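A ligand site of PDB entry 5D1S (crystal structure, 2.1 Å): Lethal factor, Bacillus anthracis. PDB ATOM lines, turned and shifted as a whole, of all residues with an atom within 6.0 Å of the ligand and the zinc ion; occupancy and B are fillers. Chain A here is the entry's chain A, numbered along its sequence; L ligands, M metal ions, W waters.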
ATOM      1  N   SER A  66       5.856 -17.944 -20.746  1.00  0.00           N
ATOM      2  CA  SER A  66       6.275 -17.574 -19.386  1.00  0.00           C
ATOM      3  C   SER A  66       5.711 -16.236 -18.912  1.00  0.00           C
ATOM      4  O   SER A  66       5.406 -15.358 -19.708  1.00  0.00           O
ATOM      5  CB  SER A  66       7.808 -17.546 -19.297  1.00  0.00           C
ATOM      6  OG  SER A  66       8.337 -18.855 -19.461  1.00  0.00           O
ATOM      7  N   ASP A  67       5.572 -16.109 -17.593  1.00  0.00           N
ATOM      8  CA  ASP A  67       5.156 -14.857 -16.948  1.00  0.00           C
ATOM      9  C   ASP A  67       6.336 -13.970 -16.662  1.00  0.00           C
ATOM     10  O   ASP A  67       6.187 -12.786 -16.370  1.00  0.00           O
ATOM     11  CB  ASP A  67       4.428 -15.123 -15.624  1.00  0.00           C
ATOM     12  CG  ASP A  67       3.143 -15.882 -15.802  1.00  0.00           C
ATOM     13  OD1 ASP A  67       2.662 -15.958 -16.951  1.00  0.00           O
ATOM     14  OD2 ASP A  67       2.602 -16.398 -14.793  1.00  0.00           O
ATOM     15  N   VAL A 392       9.437 -11.606  -9.379  1.00  0.00           N
ATOM     16  CA  VAL A 392       8.825 -11.554 -10.700  1.00  0.00           C
ATOM     17  C   VAL A 392       9.180 -10.256 -11.403  1.00  0.00           C
ATOM     18  O   VAL A 392       9.033  -9.182 -10.838  1.00  0.00           O
ATOM     19  CB  VAL A 392       7.269 -11.649 -10.647  1.00  0.00           C
ATOM     20  CG1 VAL A 392       6.666 -11.418 -12.014  1.00  0.00           C
ATOM     21  CG2 VAL A 392       6.814 -13.008 -10.090  1.00  0.00           C
ATOM     22  N   SER A 394       7.874  -8.187 -14.723  1.00  0.00           N
ATOM     23  CA  SER A 394       6.762  -8.201 -15.672  1.00  0.00           C
ATOM     24  C   SER A 394       6.278  -6.773 -15.913  1.00  0.00           C
ATOM     25  O   SER A 394       6.801  -5.842 -15.326  1.00  0.00           O
ATOM     26  CB  SER A 394       5.610  -9.078 -15.139  1.00  0.00           C
ATOM     27  OG  SER A 394       5.056  -8.567 -13.935  1.00  0.00           O
ATOM     28  N   LYS A 395       5.259  -6.597 -16.760  1.00  0.00           N
ATOM     29  CA  LYS A 395       4.730  -5.274 -17.047  1.00  0.00           C
ATOM     30  C   LYS A 395       4.083  -4.686 -15.794  1.00  0.00           C
ATOM     31  O   LYS A 395       4.214  -3.486 -15.508  1.00  0.00           O
ATOM     32  CB  LYS A 395       3.706  -5.330 -18.216  1.00  0.00           C
ATOM     33  CG  LYS A 395       2.767  -4.123 -18.300  1.00  0.00           C
ATOM     34  CD  LYS A 395       3.521  -2.784 -18.482  1.00  0.00           C
ATOM     35  CE  LYS A 395       3.970  -2.577 -19.899  1.00  0.00           C
ATOM     36  NZ  LYS A 395       4.862  -1.383 -20.119  1.00  0.00           N
ATOM     37  N   GLY A 396       3.405  -5.550 -15.050  1.00  0.00           N
ATOM     38  CA  GLY A 396       2.634  -5.113 -13.909  1.00  0.00           C
ATOM     39  C   GLY A 396       2.484  -6.177 -12.838  1.00  0.00           C
ATOM     40  O   GLY A 396       2.625  -7.370 -13.089  1.00  0.00           O
ATOM     41  N   LEU A 397       2.185  -5.721 -11.618  1.00  0.00           N
ATOM     42  CA  LEU A 397       2.167  -6.594 -10.466  1.00  0.00           C
ATOM     43  C   LEU A 397       1.315  -5.973  -9.360  1.00  0.00           C
ATOM     44  O   LEU A 397       1.344  -4.772  -9.153  1.00  0.00           O
ATOM     45  CB  LEU A 397       3.604  -6.848  -9.964  1.00  0.00           C
ATOM     46  CG  LEU A 397       3.911  -8.127  -9.174  1.00  0.00           C
ATOM     47  CD1 LEU A 397       3.780  -9.357 -10.059  1.00  0.00           C
ATOM     48  CD2 LEU A 397       5.317  -8.117  -8.531  1.00  0.00           C
ATOM     49  N   TYR A 398       0.554  -6.813  -8.675  1.00  0.00           N
ATOM     50  CA  TYR A 398      -0.043  -6.393  -7.417  1.00  0.00           C
ATOM     51  C   TYR A 398       0.557  -7.214  -6.309  1.00  0.00           C
ATOM     52  O   TYR A 398       0.602  -8.437  -6.397  1.00  0.00           O
ATOM     53  CB  TYR A 398      -1.565  -6.577  -7.412  1.00  0.00           C
ATOM     54  CG  TYR A 398      -2.187  -6.236  -6.080  1.00  0.00           C
ATOM     55  CD1 TYR A 398      -2.260  -4.922  -5.655  1.00  0.00           C
ATOM     56  CD2 TYR A 398      -2.706  -7.228  -5.245  1.00  0.00           C
ATOM     57  CE1 TYR A 398      -2.843  -4.593  -4.444  1.00  0.00           C
ATOM     58  CE2 TYR A 398      -3.299  -6.898  -4.014  1.00  0.00           C
ATOM     59  CZ  TYR A 398      -3.353  -5.576  -3.639  1.00  0.00           C
ATOM     60  OH  TYR A 398      -3.909  -5.205  -2.440  1.00  0.00           O
ATOM     61  N   LYS A 412       6.673  -4.787 -22.386  1.00  0.00           N
ATOM     62  CA  LYS A 412       5.373  -5.049 -22.972  1.00  0.00           C
ATOM     63  C   LYS A 412       4.731  -6.223 -22.258  1.00  0.00           C
ATOM     64  O   LYS A 412       5.412  -7.185 -21.897  1.00  0.00           O
ATOM     65  CB  LYS A 412       5.467  -5.336 -24.465  1.00  0.00           C
ATOM     66  CG  LYS A 412       4.111  -5.534 -25.152  1.00  0.00           C
ATOM     67  CD  LYS A 412       4.242  -6.264 -26.480  1.00  0.00           C
ATOM     68  CE  LYS A 412       4.765  -7.681 -26.290  1.00  0.00           C
ATOM     69  NZ  LYS A 412       4.929  -8.428 -27.578  1.00  0.00           N
ATOM     70  N   GLY A 413       3.419  -6.149 -22.055  1.00  0.00           N
ATOM     71  CA  GLY A 413       2.700  -7.208 -21.373  1.00  0.00           C
ATOM     72  C   GLY A 413       2.157  -8.272 -22.306  1.00  0.00           C
ATOM     73  O   GLY A 413       1.959  -8.033 -23.501  1.00  0.00           O
ATOM     74  N   VAL A 414       1.934  -9.458 -21.750  1.00  0.00           N
ATOM     75  CA  VAL A 414       1.287 -10.550 -22.469  1.00  0.00           C
ATOM     76  C   VAL A 414      -0.071 -10.113 -23.029  1.00  0.00           C
ATOM     77  O   VAL A 414      -0.991  -9.838 -22.260  1.00  0.00           O
ATOM     78  CB  VAL A 414       1.062 -11.764 -21.561  1.00  0.00           C
ATOM     79  CG1 VAL A 414       0.488 -12.926 -22.370  1.00  0.00           C
ATOM     80  CG2 VAL A 414       2.361 -12.159 -20.862  1.00  0.00           C
ATOM     81  N   GLU A 415      -0.163 -10.053 -24.350  1.00  0.00           N
ATOM     82  CA  GLU A 415      -1.418  -9.726 -25.048  1.00  0.00           C
ATOM     83  C   GLU A 415      -2.104  -8.491 -24.458  1.00  0.00           C
ATOM     84  O   GLU A 415      -3.286  -8.524 -24.093  1.00  0.00           O
ATOM     85  CB  GLU A 415      -2.363 -10.920 -25.018  1.00  0.00           C
ATOM     86  N   LEU A 416      -1.339  -7.413 -24.360  1.00  0.00           N
ATOM     87  CA  LEU A 416      -1.785  -6.164 -23.745  1.00  0.00           C
ATOM     88  C   LEU A 416      -1.619  -5.006 -24.710  1.00  0.00           C
ATOM     89  O   LEU A 416      -0.519  -4.813 -25.258  1.00  0.00           O
ATOM     90  CB  LEU A 416      -1.001  -5.907 -22.468  1.00  0.00           C
ATOM     91  CG  LEU A 416      -1.583  -4.942 -21.440  1.00  0.00           C
ATOM     92  CD1 LEU A 416      -2.938  -5.453 -20.995  1.00  0.00           C
ATOM     93  CD2 LEU A 416      -0.622  -4.839 -20.261  1.00  0.00           C
ATOM     94  N   GLU A 421      -4.408  -0.409 -19.683  1.00  0.00           N
ATOM     95  CA  GLU A 421      -5.137  -1.666 -19.495  1.00  0.00           C
ATOM     96  C   GLU A 421      -4.386  -2.542 -18.498  1.00  0.00           C
ATOM     97  O   GLU A 421      -5.013  -3.210 -17.661  1.00  0.00           O
ATOM     98  CB  GLU A 421      -5.337  -2.364 -20.837  1.00  0.00           C
ATOM     99  CG  GLU A 421      -6.349  -1.609 -21.725  1.00  0.00           C
ATOM    100  CD  GLU A 421      -6.620  -2.301 -23.057  1.00  0.00           C
ATOM    101  OE1 GLU A 421      -5.747  -3.060 -23.537  1.00  0.00           O
ATOM    102  OE2 GLU A 421      -7.725  -2.090 -23.613  1.00  0.00           O
ATOM    103  N   GLY A 422      -3.057  -2.500 -18.545  1.00  0.00           N
ATOM    104  CA  GLY A 422      -2.247  -3.204 -17.575  1.00  0.00           C
ATOM    105  C   GLY A 422      -2.561  -2.772 -16.163  1.00  0.00           C
ATOM    106  O   GLY A 422      -2.736  -3.613 -15.269  1.00  0.00           O
ATOM    107  N   PHE A 423      -2.688  -1.470 -15.966  1.00  0.00           N
ATOM    108  CA  PHE A 423      -2.970  -0.939 -14.648  1.00  0.00           C
ATOM    109  C   PHE A 423      -4.336  -1.399 -14.145  1.00  0.00           C
ATOM    110  O   PHE A 423      -4.494  -1.708 -12.961  1.00  0.00           O
ATOM    111  CB  PHE A 423      -2.892   0.578 -14.643  1.00  0.00           C
ATOM    112  CG  PHE A 423      -2.967   1.192 -13.272  1.00  0.00           C
ATOM    113  CD1 PHE A 423      -1.818   1.352 -12.509  1.00  0.00           C
ATOM    114  CD2 PHE A 423      -4.181   1.603 -12.753  1.00  0.00           C
ATOM    115  CE1 PHE A 423      -1.892   1.912 -11.247  1.00  0.00           C
ATOM    116  CE2 PHE A 423      -4.254   2.153 -11.510  1.00  0.00           C
ATOM    117  CZ  PHE A 423      -3.125   2.311 -10.757  1.00  0.00           C
ATOM    118  N   HIS A 425      -5.907  -4.107 -14.900  1.00  0.00           N
ATOM    119  CA  HIS A 425      -5.752  -5.498 -14.494  1.00  0.00           C
ATOM    120  C   HIS A 425      -5.215  -5.600 -13.060  1.00  0.00           C
ATOM    121  O   HIS A 425      -5.757  -6.353 -12.222  1.00  0.00           O
ATOM    122  CB  HIS A 425      -4.852  -6.234 -15.497  1.00  0.00           C
ATOM    123  CG  HIS A 425      -4.358  -7.563 -15.029  1.00  0.00           C
ATOM    124  ND1 HIS A 425      -4.687  -8.746 -15.662  1.00  0.00           N
ATOM    125  CD2 HIS A 425      -3.496  -7.912 -14.033  1.00  0.00           C
ATOM    126  CE1 HIS A 425      -4.069  -9.753 -15.068  1.00  0.00           C
ATOM    127  NE2 HIS A 425      -3.352  -9.278 -14.067  1.00  0.00           N
ATOM    128  N   GLU A 426      -4.169  -4.830 -12.767  1.00  0.00           N
ATOM    129  CA  GLU A 426      -3.600  -4.823 -11.417  1.00  0.00           C
ATOM    130  C   GLU A 426      -4.609  -4.303 -10.415  1.00  0.00           C
ATOM    131  O   GLU A 426      -4.699  -4.792  -9.315  1.00  0.00           O
ATOM    132  CB  GLU A 426      -2.334  -3.959 -11.362  1.00  0.00           C
ATOM    133  CG  GLU A 426      -1.328  -4.281 -12.461  1.00  0.00           C
ATOM    134  CD  GLU A 426      -0.868  -5.718 -12.439  1.00  0.00           C
ATOM    135  OE1 GLU A 426      -0.433  -6.211 -13.491  1.00  0.00           O
ATOM    136  OE2 GLU A 426      -0.931  -6.346 -11.365  1.00  0.00           O
ATOM    137  N   HIS A 429      -6.687  -7.076  -9.296  1.00  0.00           N
ATOM    138  CA  HIS A 429      -6.120  -7.860  -8.219  1.00  0.00           C
ATOM    139  C   HIS A 429      -6.427  -7.220  -6.884  1.00  0.00           C
ATOM    140  O   HIS A 429      -6.740  -7.895  -5.894  1.00  0.00           O
ATOM    141  CB  HIS A 429      -4.593  -8.001  -8.394  1.00  0.00           C
ATOM    142  CG  HIS A 429      -4.191  -8.987  -9.438  1.00  0.00           C
ATOM    143  ND1 HIS A 429      -4.734 -10.252  -9.513  1.00  0.00           N
ATOM    144  CD2 HIS A 429      -3.286  -8.900 -10.439  1.00  0.00           C
ATOM    145  CE1 HIS A 429      -4.169 -10.906 -10.522  1.00  0.00           C
ATOM    146  NE2 HIS A 429      -3.304 -10.107 -11.107  1.00  0.00           N
ATOM    147  N   TYR A 467      -4.264 -15.783 -21.417  1.00  0.00           N
ATOM    148  CA  TYR A 467      -3.497 -15.598 -20.187  1.00  0.00           C
ATOM    149  C   TYR A 467      -4.377 -15.876 -18.980  1.00  0.00           C
ATOM    150  O   TYR A 467      -3.900 -16.336 -17.952  1.00  0.00           O
ATOM    151  CB  TYR A 467      -2.901 -14.188 -20.078  1.00  0.00           C
ATOM    152  CG  TYR A 467      -2.201 -14.004 -18.757  1.00  0.00           C
ATOM    153  CD1 TYR A 467      -1.072 -14.743 -18.443  1.00  0.00           C
ATOM    154  CD2 TYR A 467      -2.691 -13.117 -17.808  1.00  0.00           C
ATOM    155  CE1 TYR A 467      -0.433 -14.595 -17.210  1.00  0.00           C
ATOM    156  CE2 TYR A 467      -2.052 -12.960 -16.575  1.00  0.00           C
ATOM    157  CZ  TYR A 467      -0.923 -13.699 -16.281  1.00  0.00           C
ATOM    158  OH  TYR A 467      -0.305 -13.542 -15.057  1.00  0.00           O
ATOM    159  N   ALA A 473      -6.941 -16.111  -9.654  1.00  0.00           N
ATOM    160  CA  ALA A 473      -6.622 -14.714  -9.449  1.00  0.00           C
ATOM    161  C   ALA A 473      -6.450 -13.988 -10.789  1.00  0.00           C
ATOM    162  O   ALA A 473      -6.887 -12.845 -10.941  1.00  0.00           O
ATOM    163  CB  ALA A 473      -5.340 -14.563  -8.589  1.00  0.00           C
ATOM    164  N   GLU A 474      -5.804 -14.637 -11.750  1.00  0.00           N
ATOM    165  CA  GLU A 474      -5.525 -14.003 -13.028  1.00  0.00           C
ATOM    166  C   GLU A 474      -6.807 -13.983 -13.875  1.00  0.00           C
ATOM    167  O   GLU A 474      -7.096 -12.990 -14.555  1.00  0.00           O
ATOM    168  CB  GLU A 474      -4.399 -14.728 -13.765  1.00  0.00           C
ATOM    169  CG  GLU A 474      -3.102 -14.879 -12.974  1.00  0.00           C
ATOM    170  CD  GLU A 474      -2.406 -13.557 -12.654  1.00  0.00           C
ATOM    171  OE1 GLU A 474      -2.885 -12.496 -13.093  1.00  0.00           O
ATOM    172  OE2 GLU A 474      -1.368 -13.586 -11.963  1.00  0.00           O
ATOM    173  N   ALA A 477      -8.823 -11.109 -12.716  1.00  0.00           N
ATOM    174  CA  ALA A 477      -8.189  -9.855 -13.113  1.00  0.00           C
ATOM    175  C   ALA A 477      -8.376  -9.565 -14.601  1.00  0.00           C
ATOM    176  O   ALA A 477      -8.666  -8.442 -14.975  1.00  0.00           O
ATOM    177  CB  ALA A 477      -6.689  -9.850 -12.752  1.00  0.00           C
ATOM    178  N   GLU A 478      -8.188 -10.585 -15.429  1.00  0.00           N
ATOM    179  CA  GLU A 478      -8.426 -10.447 -16.850  1.00  0.00           C
ATOM    180  C   GLU A 478      -9.902 -10.127 -17.133  1.00  0.00           C
ATOM    181  O   GLU A 478     -10.219  -9.219 -17.900  1.00  0.00           O
ATOM    182  CB  GLU A 478      -7.973 -11.700 -17.596  1.00  0.00           C
ATOM    183  CG  GLU A 478      -6.451 -11.762 -17.803  1.00  0.00           C
ATOM    184  CD  GLU A 478      -5.950 -10.653 -18.713  1.00  0.00           C
ATOM    185  OE1 GLU A 478      -5.598 -10.944 -19.870  1.00  0.00           O
ATOM    186  OE2 GLU A 478      -5.935  -9.475 -18.274  1.00  0.00           O
ATOM    187  N   ARG A 481     -10.493  -6.639 -16.154  1.00  0.00           N
ATOM    188  CA  ARG A 481      -9.922  -5.729 -17.128  1.00  0.00           C
ATOM    189  C   ARG A 481     -10.848  -5.571 -18.326  1.00  0.00           C
ATOM    190  O   ARG A 481     -11.178  -4.460 -18.719  1.00  0.00           O
ATOM    191  CB  ARG A 481      -8.564  -6.211 -17.597  1.00  0.00           C
ATOM    192  CG  ARG A 481      -8.051  -5.431 -18.776  1.00  0.00           C
ATOM    193  CD  ARG A 481      -6.626  -5.784 -19.101  1.00  0.00           C
ATOM    194  NE  ARG A 481      -6.505  -7.109 -19.677  1.00  0.00           N
ATOM    195  CZ  ARG A 481      -6.668  -7.383 -20.965  1.00  0.00           C
ATOM    196  NH1 ARG A 481      -6.980  -6.417 -21.824  1.00  0.00           N
ATOM    197  NH2 ARG A 481      -6.519  -8.622 -21.405  1.00  0.00           N
HETATM  198  C1  LIG L   1       1.826 -10.257 -14.764  1.00  0.00           C
HETATM  199  C2  LIG L   1       0.528 -10.211 -13.950  1.00  0.00           C
HETATM  200  O1  LIG L   1      -0.552  -8.851 -12.265  1.00  0.00           O
HETATM  201  N1  LIG L   1       1.833 -10.248 -16.255  1.00  0.00           N
HETATM  202  C3  LIG L   1       0.387  -8.412 -17.373  1.00  0.00           C
HETATM  203  C4  LIG L   1      -0.416  -8.962 -18.389  1.00  0.00           C
HETATM  204  C5  LIG L   1      -1.727  -8.500 -18.570  1.00  0.00           C
HETATM  205  C6  LIG L   1      -2.206  -7.486 -17.736  1.00  0.00           C
HETATM  206  C7  LIG L   1      -1.414  -6.937 -16.739  1.00  0.00           C
HETATM  207  C8  LIG L   1      -0.112  -7.400 -16.558  1.00  0.00           C
HETATM  208  C9  LIG L   1       1.829 -11.534 -16.941  1.00  0.00           C
HETATM  209  C10 LIG L   1       2.624 -11.457 -14.227  1.00  0.00           C
HETATM  210  N2  LIG L   1       0.478  -9.164 -13.135  1.00  0.00           N
HETATM  211  O2  LIG L   1      -0.367 -11.064 -13.972  1.00  0.00           O
HETATM  212  S1  LIG L   1       1.893  -8.942 -17.143  1.00  0.00           S
HETATM  213  O3  LIG L   1       2.486  -9.114 -18.450  1.00  0.00           O
HETATM  214  O4  LIG L   1       2.664  -7.934 -16.453  1.00  0.00           O
HETATM  215  F1  LIG L   1      -3.457  -7.030 -17.907  1.00  0.00           F
HETATM  216  C11 LIG L   1      -2.631  -9.068 -19.643  1.00  0.00           C
HETATM  217 ZN    ZN M   1      -2.065 -10.505 -12.758  1.00  0.00          ZN
HETATM  218  O   HOH W   1       0.195  -9.648  -9.800  1.00  0.00           O
HETATM  219  O   HOH W   2      -4.057 -11.022 -22.039  1.00  0.00           O
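The side-chain carboxylate (OE1) of Glu 426 sits at hydrogen-bond distance from a nitrogen (N2) of the ligand, 3.1 Å away.
OH of Tyr 467 lies close to O2 of the ligand, 2.7 Å away.
N of Gly 396 sits at hydrogen-bond distance from O4 of the ligand (2.9 Å).
O of Gly 396 lies within hydrogen-bond range of N2 of the ligand (2.8 Å).
The backbone NH (N) of Lys 395 is in hydrogen-bond range of an oxygen (O4) of the ligand (2.9 Å).
The backbone NH of Val 414 lies within hydrogen-bond range of an oxygen (O3) of the ligand (3.4 Å).
OH of Tyr 467 sits close to OE2 of Glu 474 (3.3 Å).
The side-chain carboxylate (OE2) of Glu 478 is in hydrogen-bond range of a ring nitrogen (ND1) of His 425 (3.0 Å).
The backbone NH of Leu 397 sits close to the side-chain carboxylate of Glu 426 (3.2 Å).
The backbone NH (N) of Tyr 398 lies within hydrogen-bond range of the side-chain carboxylate (OE2) of Glu 426, 3.1 Å away.
OG of Ser 394 is in hydrogen-bond range of O of Gly 396, 2.8 Å away.
NE of Arg 481 is in salt-bridge range of OE2 of Glu 478, 2.8 Å away.
The guanidinium group (NH1) of Arg 481 lies within salt-bridge range of the side-chain carboxylate (OE1) of Glu 421, at 3.97 Å.
Merely in contact with the ligand: Ser 394, Gly 413, Glu 478, Leu 416, Arg 481, Gly 422 and Leu 397.
15 residues have an atom within 4 Å of the ligand: Ser 394, Lys 395, Gly 396, Leu 397, Gly 413, Val 414, Leu 416, Gly 422, His 425, Glu 426, His 429, Tyr 467, Glu 474, Glu 478 and Arg 481.
Along chain A the residues within 4 Å of the ligand span positions 394 to 481.
The nearest printed residue that does not touch the ligand is Glu 421 (4.1 Å).
Of the 25 residues printed, 3 come within 4 Å of the zinc ion.
The zinc ion is bound by a ring nitrogen (NE2) of His 429, an oxygen (O2) of the ligand, the side-chain carboxylate of Glu 474, a ring nitrogen (NE2) of His 425 and an oxygen (O1) of the ligand.
The zinc ion has five donor atoms within binding distance.
Water W1 bridges N of Tyr 398 (3.1 Å) and N2 of the ligand (3.4 Å).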
